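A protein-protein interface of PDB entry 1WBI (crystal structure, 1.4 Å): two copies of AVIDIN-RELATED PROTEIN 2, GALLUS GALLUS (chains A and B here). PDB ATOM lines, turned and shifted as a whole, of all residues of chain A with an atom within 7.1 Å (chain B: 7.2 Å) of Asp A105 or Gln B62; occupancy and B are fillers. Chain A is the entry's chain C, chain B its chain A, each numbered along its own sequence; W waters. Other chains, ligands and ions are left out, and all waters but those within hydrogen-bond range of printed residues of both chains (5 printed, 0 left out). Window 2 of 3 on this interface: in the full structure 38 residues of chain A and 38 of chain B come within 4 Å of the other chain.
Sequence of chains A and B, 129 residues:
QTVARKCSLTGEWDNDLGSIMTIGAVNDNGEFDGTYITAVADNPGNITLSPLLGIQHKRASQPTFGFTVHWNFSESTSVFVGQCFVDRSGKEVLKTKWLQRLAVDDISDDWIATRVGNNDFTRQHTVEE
OG1 of Thr B64 is in hydrogen-bond range of O of Glu A75 (2.6 Å).
The side-chain amide nitrogen (NE2) of Gln B83 lies within hydrogen-bond range of the backbone carbonyl oxygen (O) of Val A104 (2.9 Å).
A ring nitrogen (NE2) of His B57 is in hydrogen-bond range of the backbone carbonyl oxygen (O) of Glu A75 (3.4 Å).
NE2 of Gln B62 lies within hydrogen-bond range of O of Asp A105, 2.9 Å away.
OE1 of Gln B62 is in hydrogen-bond range of N of Val B86, at 3.0 Å.
NH2 of Arg B5 sits at hydrogen-bond distance from O of Ala B60 (3.3 Å).
N of His B57 sits at hydrogen-bond distance from O of Thr B64 (3.0 Å).
The side-chain carboxylate (OD2) of Asp A106 lies within hydrogen-bond range of the side-chain hydroxyl (OG) of Ser A108 (2.7 Å).
O of Gln B62 lies within hydrogen-bond range of NE2 of Gln B83 (2.8 Å).
SG of Cys B7 is disulfide-bonded to SG of Cys B84, 2.1 Å away.
Ala B60 touches Glu A75 (CB to OE1, 3.7 Å).
Ala A103 touches Thr B64.
Gln B83 touches Ala A103.
Phe B85 touches Val A104 (CZ to CG2, 3.8 Å).
Phe B85 touches Asp A106.
Phe B85 touches Ile A107 (CD1 to N, 3.4 Å).
Of the printed residues of chain B, Asp A105 touches Gln B62.
Of chain A, only Asp A105 comes within 4 Å of Gln B62.
Of the printed residues of chain B, Asp A106 touches Phe B85.
Printed residues of chain A within 4 Å of Ala B60: Glu A75.
Of the printed residues of chain B, Val A104 touches Gln B83 and Phe B85.
Of the printed residues of chain A, His B57 touches Glu A75 (3.4 Å).
Ser B61 touches none of the printed residues of chain A.
The nearest residue of chain A that does not touch Gln B62 is Asp A106 (4.4 Å).
The nearest printed residue of chain B that does not touch Asp A106 is Gln B62 (4.4 Å).
Of the 8 printed residues of chain A, 6 touch a printed residue of chain B.
Printed residues of chain A that touch a printed residue of chain B: Glu A75, Ala A103, Val A104, Asp A105, Asp A106 and Ile A107.
Hydrophobic or aromatic side chains of chain A that line the printed part of chain B: Val A104 and Ile A107.
Along chain A the printed residues that touch a printed residue of chain B span positions 75 to 107.
Of the 17 printed residues of chain B, 6 touch a printed residue of chain A.
Hydrophobic or aromatic side chains of chain B within 4 Å of the printed part of chain A: His B57, Ala B60 and Phe B85.
Among the printed residues, 10 pairs touch across the chains.
Among the printed residues, no Asp or Glu carboxylate lies within 4 Å of a Lys or Arg side-chain nitrogen of the other chain.
No position is printed for both chains.
Water W4 lies within hydrogen-bond range of the side-chain carboxylate (OE1) of Glu A75 (2.7 Å) and the backbone NH (N) of Thr B64 (3.0 Å).
Water W1 lies within hydrogen-bond range of the side-chain carboxylate of Asp A106 (2.8 Å), the side-chain amide oxygen of Gln B62 (2.8 Å) and the backbone NH of Ile A107 (3.1 Å).
Water W3 lies within hydrogen-bond range of OE1 of Glu A75 (2.9 Å), N of Ala B60 (2.9 Å) and N of Arg B59 (3.3 Å).
Water W2 lies within hydrogen-bond range of the backbone carbonyl oxygen (O) of Asp A105 (2.9 Å), the side-chain carboxylate (OD1) of Asp A106 (3.1 Å) and the side-chain amide nitrogen (NE2) of Gln B62 (3.3 Å).
Water W5 bridges the backbone carbonyl oxygen (O) of Val A104 (2.9 Å) and the side-chain amide nitrogen (NE2) of Gln B62 (3.1 Å).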
ATOM      1  N   GLU A  75      -3.968  -8.827 -30.713  1.00  0.00           N
ATOM      2  CA  GLU A  75      -4.827  -8.759 -29.531  1.00  0.00           C
ATOM      3  C   GLU A  75      -5.713  -7.522 -29.515  1.00  0.00           C
ATOM      4  O   GLU A  75      -6.436  -7.295 -28.535  1.00  0.00           O
ATOM      5  CB  GLU A  75      -4.003  -8.872 -28.280  1.00  0.00           C
ATOM      6  CG  GLU A  75      -3.397 -10.262 -28.147  1.00  0.00           C
ATOM      7  CD  GLU A  75      -4.373 -11.375 -27.874  1.00  0.00           C
ATOM      8  OE1 GLU A  75      -5.509 -11.191 -27.338  1.00  0.00           O
ATOM      9  OE2 GLU A  75      -3.964 -12.514 -28.217  1.00  0.00           O
ATOM     10  N   ALA A 103      -3.697  -3.890 -26.832  1.00  0.00           N
ATOM     11  CA  ALA A 103      -3.508  -4.587 -25.574  1.00  0.00           C
ATOM     12  C   ALA A 103      -2.254  -4.106 -24.877  1.00  0.00           C
ATOM     13  O   ALA A 103      -1.161  -4.062 -25.504  1.00  0.00           O
ATOM     14  CB  ALA A 103      -3.401  -6.042 -25.823  1.00  0.00           C
ATOM     15  N   VAL A 104      -2.358  -3.729 -23.612  1.00  0.00           N
ATOM     16  CA  VAL A 104      -1.187  -3.432 -22.823  1.00  0.00           C
ATOM     17  C   VAL A 104      -1.081  -4.418 -21.676  1.00  0.00           C
ATOM     18  O   VAL A 104      -2.022  -5.124 -21.337  1.00  0.00           O
ATOM     19  CB  VAL A 104      -1.123  -1.933 -22.344  1.00  0.00           C
ATOM     20  CG1 VAL A 104      -1.062  -0.986 -23.548  1.00  0.00           C
ATOM     21  CG2 VAL A 104      -2.359  -1.615 -21.505  1.00  0.00           C
ATOM     22  N   ASP A 105       0.084  -4.409 -21.058  1.00  0.00           N
ATOM     23  CA  ASP A 105       0.428  -5.391 -20.049  1.00  0.00           C
ATOM     24  C   ASP A 105      -0.218  -5.126 -18.689  1.00  0.00           C
ATOM     25  O   ASP A 105      -0.472  -6.042 -17.915  1.00  0.00           O
ATOM     26  CB  ASP A 105       1.947  -5.373 -19.882  1.00  0.00           C
ATOM     27  CG  ASP A 105       2.681  -5.970 -21.091  1.00  0.00           C
ATOM     28  OD1 ASP A 105       2.107  -6.861 -21.778  1.00  0.00           O
ATOM     29  OD2 ASP A 105       3.851  -5.586 -21.324  1.00  0.00           O
ATOM     30  N   ASP A 106      -0.413  -3.865 -18.353  1.00  0.00           N
ATOM     31  CA  ASP A 106      -0.974  -3.543 -17.047  1.00  0.00           C
ATOM     32  C   ASP A 106      -1.860  -2.335 -17.104  1.00  0.00           C
ATOM     33  O   ASP A 106      -1.671  -1.474 -17.996  1.00  0.00           O
ATOM     34  CB  ASP A 106       0.163  -3.295 -16.073  1.00  0.00           C
ATOM     35  CG  ASP A 106      -0.321  -3.144 -14.655  1.00  0.00           C
ATOM     36  OD1 ASP A 106      -0.827  -4.170 -14.080  1.00  0.00           O
ATOM     37  OD2 ASP A 106      -0.214  -1.996 -14.151  1.00  0.00           O
ATOM     38  N   ILE A 107      -2.825  -2.281 -16.178  1.00  0.00           N
ATOM     39  CA  ILE A 107      -3.741  -1.139 -16.067  1.00  0.00           C
ATOM     40  C   ILE A 107      -3.011   0.222 -16.028  1.00  0.00           C
ATOM     41  O   ILE A 107      -3.525   1.206 -16.562  1.00  0.00           O
ATOM     42  CB  ILE A 107      -4.697  -1.328 -14.874  1.00  0.00           C
ATOM     43  CG1 ILE A 107      -5.897  -0.385 -14.970  1.00  0.00           C
ATOM     44  CG2 ILE A 107      -3.983  -1.235 -13.535  1.00  0.00           C
ATOM     45  CD1 ILE A 107      -7.045  -0.772 -14.070  1.00  0.00           C
ATOM     46  N   SER A 108      -1.801   0.278 -15.456  1.00  0.00           N
ATOM     47  CA  SER A 108      -1.002   1.515 -15.417  1.00  0.00           C
ATOM     48  C   SER A 108      -0.567   2.058 -16.791  1.00  0.00           C
ATOM     49  O   SER A 108      -0.250   3.246 -16.912  1.00  0.00           O
ATOM     50  CB  SER A 108       0.236   1.319 -14.534  1.00  0.00           C
ATOM     51  OG  SER A 108       1.017   0.229 -14.996  1.00  0.00           O
ATOM     52  N   ASP A 109      -0.548   1.186 -17.806  1.00  0.00           N
ATOM     53  CA  ASP A 109      -0.201   1.566 -19.178  1.00  0.00           C
ATOM     54  C   ASP A 109      -1.414   1.980 -20.002  1.00  0.00           C
ATOM     55  O   ASP A 109      -1.254   2.254 -21.181  1.00  0.00           O
ATOM     56  CB  ASP A 109       0.433   0.378 -19.909  1.00  0.00           C
ATOM     57  CG  ASP A 109       1.605  -0.206 -19.169  1.00  0.00           C
ATOM     58  OD1 ASP A 109       2.493   0.601 -18.796  1.00  0.00           O
ATOM     59  OD2 ASP A 109       1.611  -1.465 -19.000  1.00  0.00           O
ATOM     60  N   ARG B   5     -14.597 -17.382 -15.811  1.00  0.00           N
ATOM     61  CA  ARG B   5     -13.278 -16.769 -15.854  1.00  0.00           C
ATOM     62  C   ARG B   5     -13.356 -15.289 -15.537  1.00  0.00           C
ATOM     63  O   ARG B   5     -14.318 -14.613 -15.912  1.00  0.00           O
ATOM     64  CB  ARG B   5     -12.678 -16.854 -17.274  1.00  0.00           C
ATOM     65  CG  ARG B   5     -11.849 -18.049 -17.570  1.00  0.00           C
ATOM     66  CD  ARG B   5     -11.449 -18.077 -19.002  1.00  0.00           C
ATOM     67  NE  ARG B   5     -10.524 -17.000 -19.383  1.00  0.00           N
ATOM     68  CZ  ARG B   5      -9.316 -17.180 -19.916  1.00  0.00           C
ATOM     69  NH1 ARG B   5      -8.814 -18.399 -20.104  1.00  0.00           N
ATOM     70  NH2 ARG B   5      -8.572 -16.123 -20.215  1.00  0.00           N
ATOM     71  N   LYS B   6     -12.312 -14.765 -14.922  1.00  0.00           N
ATOM     72  CA  LYS B   6     -12.139 -13.309 -14.825  1.00  0.00           C
ATOM     73  C   LYS B   6     -12.108 -12.717 -16.231  1.00  0.00           C
ATOM     74  O   LYS B   6     -11.537 -13.298 -17.149  1.00  0.00           O
ATOM     75  CB  LYS B   6     -10.848 -12.970 -14.075  1.00  0.00           C
ATOM     76  CG  LYS B   6     -10.838 -13.360 -12.613  1.00  0.00           C
ATOM     77  CD  LYS B   6     -11.863 -12.634 -11.754  1.00  0.00           C
ATOM     78  CE  LYS B   6     -11.729 -13.041 -10.292  1.00  0.00           C
ATOM     79  NZ  LYS B   6     -12.552 -12.105  -9.454  1.00  0.00           N
ATOM     80  N   CYS B   7     -12.703 -11.552 -16.388  1.00  0.00           N
ATOM     81  CA  CYS B   7     -12.770 -10.846 -17.675  1.00  0.00           C
ATOM     82  C   CYS B   7     -13.561 -11.573 -18.769  1.00  0.00           C
ATOM     83  O   CYS B   7     -13.453 -11.234 -19.967  1.00  0.00           O
ATOM     84  CB  CYS B   7     -11.376 -10.410 -18.156  1.00  0.00           C
ATOM     85  SG  CYS B   7     -10.681  -9.146 -17.166  1.00  0.00           S
ATOM     86  N   HIS B  57     -11.913 -10.645 -27.086  1.00  0.00           N
ATOM     87  CA  HIS B  57     -10.904 -11.709 -27.146  1.00  0.00           C
ATOM     88  C   HIS B  57     -11.120 -12.677 -25.981  1.00  0.00           C
ATOM     89  O   HIS B  57     -11.442 -12.265 -24.896  1.00  0.00           O
ATOM     90  CB  HIS B  57      -9.503 -11.105 -27.143  1.00  0.00           C
ATOM     91  CG  HIS B  57      -9.154 -10.461 -28.434  1.00  0.00           C
ATOM     92  ND1 HIS B  57      -8.476 -11.130 -29.434  1.00  0.00           N
ATOM     93  CD2 HIS B  57      -9.365  -9.202 -28.901  1.00  0.00           C
ATOM     94  CE1 HIS B  57      -8.335 -10.318 -30.471  1.00  0.00           C
ATOM     95  NE2 HIS B  57      -8.833  -9.140 -30.164  1.00  0.00           N
ATOM     96  N   ARG B  59      -8.883 -15.688 -25.045  1.00  0.00           N
ATOM     97  CA  ARG B  59      -7.759 -16.369 -24.394  1.00  0.00           C
ATOM     98  C   ARG B  59      -6.955 -15.493 -23.476  1.00  0.00           C
ATOM     99  O   ARG B  59      -6.397 -15.956 -22.485  1.00  0.00           O
ATOM    100  CB  ARG B  59      -6.857 -16.988 -25.449  1.00  0.00           C
ATOM    101  CG  ARG B  59      -7.430 -18.243 -26.003  1.00  0.00           C
ATOM    102  CD  ARG B  59      -6.582 -18.738 -27.141  1.00  0.00           C
ATOM    103  NE  ARG B  59      -6.933 -18.018 -28.344  1.00  0.00           N
ATOM    104  CZ  ARG B  59      -6.290 -18.161 -29.495  1.00  0.00           C
ATOM    105  NH1 ARG B  59      -5.219 -18.932 -29.584  1.00  0.00           N
ATOM    106  NH2 ARG B  59      -6.705 -17.494 -30.563  1.00  0.00           N
ATOM    107  N   ALA B  60      -6.843 -14.211 -23.814  1.00  0.00           N
ATOM    108  CA  ALA B  60      -5.957 -13.323 -23.085  1.00  0.00           C
ATOM    109  C   ALA B  60      -6.357 -13.202 -21.616  1.00  0.00           C
ATOM    110  O   ALA B  60      -7.537 -13.169 -21.317  1.00  0.00           O
ATOM    111  CB  ALA B  60      -5.969 -11.950 -23.758  1.00  0.00           C
ATOM    112  N   SER B  61      -5.390 -13.128 -20.707  1.00  0.00           N
ATOM    113  CA  SER B  61      -5.709 -12.920 -19.293  1.00  0.00           C
ATOM    114  C   SER B  61      -6.375 -11.562 -19.058  1.00  0.00           C
ATOM    115  O   SER B  61      -7.217 -11.464 -18.139  1.00  0.00           O
ATOM    116  CB  SER B  61      -4.465 -13.015 -18.422  1.00  0.00           C
ATOM    117  OG  SER B  61      -3.569 -12.010 -18.712  1.00  0.00           O
ATOM    118  N   GLN B  62      -6.041 -10.570 -19.893  1.00  0.00           N
ATOM    119  CA  GLN B  62      -6.580  -9.185 -19.800  1.00  0.00           C
ATOM    120  C   GLN B  62      -7.024  -8.761 -21.193  1.00  0.00           C
ATOM    121  O   GLN B  62      -6.315  -8.023 -21.875  1.00  0.00           O
ATOM    122  CB  GLN B  62      -5.554  -8.229 -19.183  1.00  0.00           C
ATOM    123  CG  GLN B  62      -5.177  -8.623 -17.764  1.00  0.00           C
ATOM    124  CD  GLN B  62      -4.269  -7.642 -17.032  1.00  0.00           C
ATOM    125  OE1 GLN B  62      -4.622  -7.139 -15.971  1.00  0.00           O
ATOM    126  NE2 GLN B  62      -3.095  -7.337 -17.617  1.00  0.00           N
ATOM    127  N   PRO B  63      -8.188  -9.276 -21.647  1.00  0.00           N
ATOM    128  CA  PRO B  63      -8.597  -9.150 -23.048  1.00  0.00           C
ATOM    129  C   PRO B  63      -9.083  -7.774 -23.461  1.00  0.00           C
ATOM    130  O   PRO B  63      -9.627  -7.044 -22.628  1.00  0.00           O
ATOM    131  CB  PRO B  63      -9.744 -10.154 -23.171  1.00  0.00           C
ATOM    132  CG  PRO B  63     -10.358 -10.134 -21.779  1.00  0.00           C
ATOM    133  CD  PRO B  63      -9.144 -10.092 -20.883  1.00  0.00           C
ATOM    134  N   THR B  64      -8.877  -7.413 -24.720  1.00  0.00           N
ATOM    135  CA  THR B  64      -9.573  -6.291 -25.315  1.00  0.00           C
ATOM    136  C   THR B  64     -10.944  -6.723 -25.810  1.00  0.00           C
ATOM    137  O   THR B  64     -11.206  -7.937 -26.046  1.00  0.00           O
ATOM    138  CB  THR B  64      -8.768  -5.578 -26.454  1.00  0.00           C
ATOM    139  OG1 THR B  64      -8.724  -6.420 -27.625  1.00  0.00           O
ATOM    140  CG2 THR B  64      -7.380  -5.246 -26.010  1.00  0.00           C
ATOM    141  N   GLY B  82     -12.225  -1.269 -25.262  1.00  0.00           N
ATOM    142  CA  GLY B  82     -11.405  -1.221 -24.094  1.00  0.00           C
ATOM    143  C   GLY B  82     -10.719  -2.510 -23.771  1.00  0.00           C
ATOM    144  O   GLY B  82     -10.598  -3.391 -24.638  1.00  0.00           O
ATOM    145  N   GLN B  83     -10.123  -2.541 -22.583  1.00  0.00           N
ATOM    146  CA  GLN B  83      -9.448  -3.718 -22.057  1.00  0.00           C
ATOM    147  C   GLN B  83      -9.926  -3.985 -20.649  1.00  0.00           C
ATOM    148  O   GLN B  83     -10.138  -3.070 -19.859  1.00  0.00           O
ATOM    149  CB  GLN B  83      -7.918  -3.516 -22.144  1.00  0.00           C
ATOM    150  CG  GLN B  83      -7.084  -4.779 -21.835  1.00  0.00           C
ATOM    151  CD  GLN B  83      -5.598  -4.587 -22.085  1.00  0.00           C
ATOM    152  OE1 GLN B  83      -5.146  -3.527 -22.511  1.00  0.00           O
ATOM    153  NE2 GLN B  83      -4.805  -5.614 -21.767  1.00  0.00           N
ATOM    154  N   CYS B  84     -10.063  -5.266 -20.366  1.00  0.00           N
ATOM    155  CA  CYS B  84     -10.409  -5.760 -19.041  1.00  0.00           C
ATOM    156  C   CYS B  84      -9.136  -6.131 -18.301  1.00  0.00           C
ATOM    157  O   CYS B  84      -8.341  -6.914 -18.838  1.00  0.00           O
ATOM    158  CB  CYS B  84     -11.317  -6.978 -19.145  1.00  0.00           C
ATOM    159  SG  CYS B  84     -11.937  -7.532 -17.505  1.00  0.00           S
ATOM    160  N   PHE B  85      -8.882  -5.470 -17.183  1.00  0.00           N
ATOM    161  CA  PHE B  85      -7.746  -5.732 -16.325  1.00  0.00           C
ATOM    162  C   PHE B  85      -8.154  -6.466 -15.066  1.00  0.00           C
ATOM    163  O   PHE B  85      -9.276  -6.284 -14.590  1.00  0.00           O
ATOM    164  CB  PHE B  85      -7.053  -4.433 -16.003  1.00  0.00           C
ATOM    165  CG  PHE B  85      -6.468  -3.739 -17.199  1.00  0.00           C
ATOM    166  CD1 PHE B  85      -5.223  -4.116 -17.718  1.00  0.00           C
ATOM    167  CD2 PHE B  85      -7.141  -2.701 -17.799  1.00  0.00           C
ATOM    168  CE1 PHE B  85      -4.685  -3.458 -18.806  1.00  0.00           C
ATOM    169  CE2 PHE B  85      -6.617  -2.012 -18.862  1.00  0.00           C
ATOM    170  CZ  PHE B  85      -5.382  -2.394 -19.401  1.00  0.00           C
ATOM    171  N   VAL B  86      -7.239  -7.264 -14.540  1.00  0.00           N
ATOM    172  CA  VAL B  86      -7.499  -8.026 -13.306  1.00  0.00           C
ATOM    173  C   VAL B  86      -6.328  -7.773 -12.365  1.00  0.00           C
ATOM    174  O   VAL B  86      -5.202  -8.074 -12.725  1.00  0.00           O
ATOM    175  CB  VAL B  86      -7.606  -9.532 -13.568  1.00  0.00           C
ATOM    176  CG1 VAL B  86      -8.017 -10.251 -12.283  1.00  0.00           C
ATOM    177  CG2 VAL B  86      -8.599  -9.838 -14.654  1.00  0.00           C
ATOM    178  N   ASP B  87      -6.571  -7.217 -11.178  1.00  0.00           N
ATOM    179  CA  ASP B  87      -5.503  -7.018 -10.224  1.00  0.00           C
ATOM    180  C   ASP B  87      -5.231  -8.319  -9.431  1.00  0.00           C
ATOM    181  O   ASP B  87      -5.923  -9.312  -9.597  1.00  0.00           O
ATOM    182  CB  ASP B  87      -5.737  -5.741  -9.360  1.00  0.00           C
ATOM    183  CG  ASP B  87      -6.779  -5.892  -8.302  1.00  0.00           C
ATOM    184  OD1 ASP B  87      -7.157  -7.031  -7.936  1.00  0.00           O
ATOM    185  OD2 ASP B  87      -7.183  -4.814  -7.761  1.00  0.00           O
ATOM    186  N   LYS B  91      -9.781  -8.227  -8.673  1.00  0.00           N
ATOM    187  CA  LYS B  91     -10.708  -7.170  -9.064  1.00  0.00           C
ATOM    188  C   LYS B  91     -10.574  -6.832 -10.549  1.00  0.00           C
ATOM    189  O   LYS B  91      -9.485  -6.513 -11.022  1.00  0.00           O
ATOM    190  CB  LYS B  91     -10.525  -5.917  -8.208  1.00  0.00           C
ATOM    191  CG  LYS B  91     -11.520  -4.816  -8.578  1.00  0.00           C
ATOM    192  CD  LYS B  91     -11.288  -3.546  -7.785  1.00  0.00           C
ATOM    193  CE  LYS B  91     -12.252  -2.444  -8.213  1.00  0.00           C
ATOM    194  NZ  LYS B  91     -12.012  -2.032  -9.595  1.00  0.00           N
HETATM  195  O   HOH W   1      -3.486  -4.919 -14.649  1.00  0.00           O
HETATM  196  O   HOH W   2      -0.748  -7.072 -15.245  1.00  0.00           O
HETATM  197  O   HOH W   3      -6.951 -13.576 -26.633  1.00  0.00           O
HETATM  198  O   HOH W   4      -6.961  -9.065 -26.403  1.00  0.00           O
HETATM  199  O   HOH W   5      -2.123  -7.939 -20.473  1.00  0.00           O
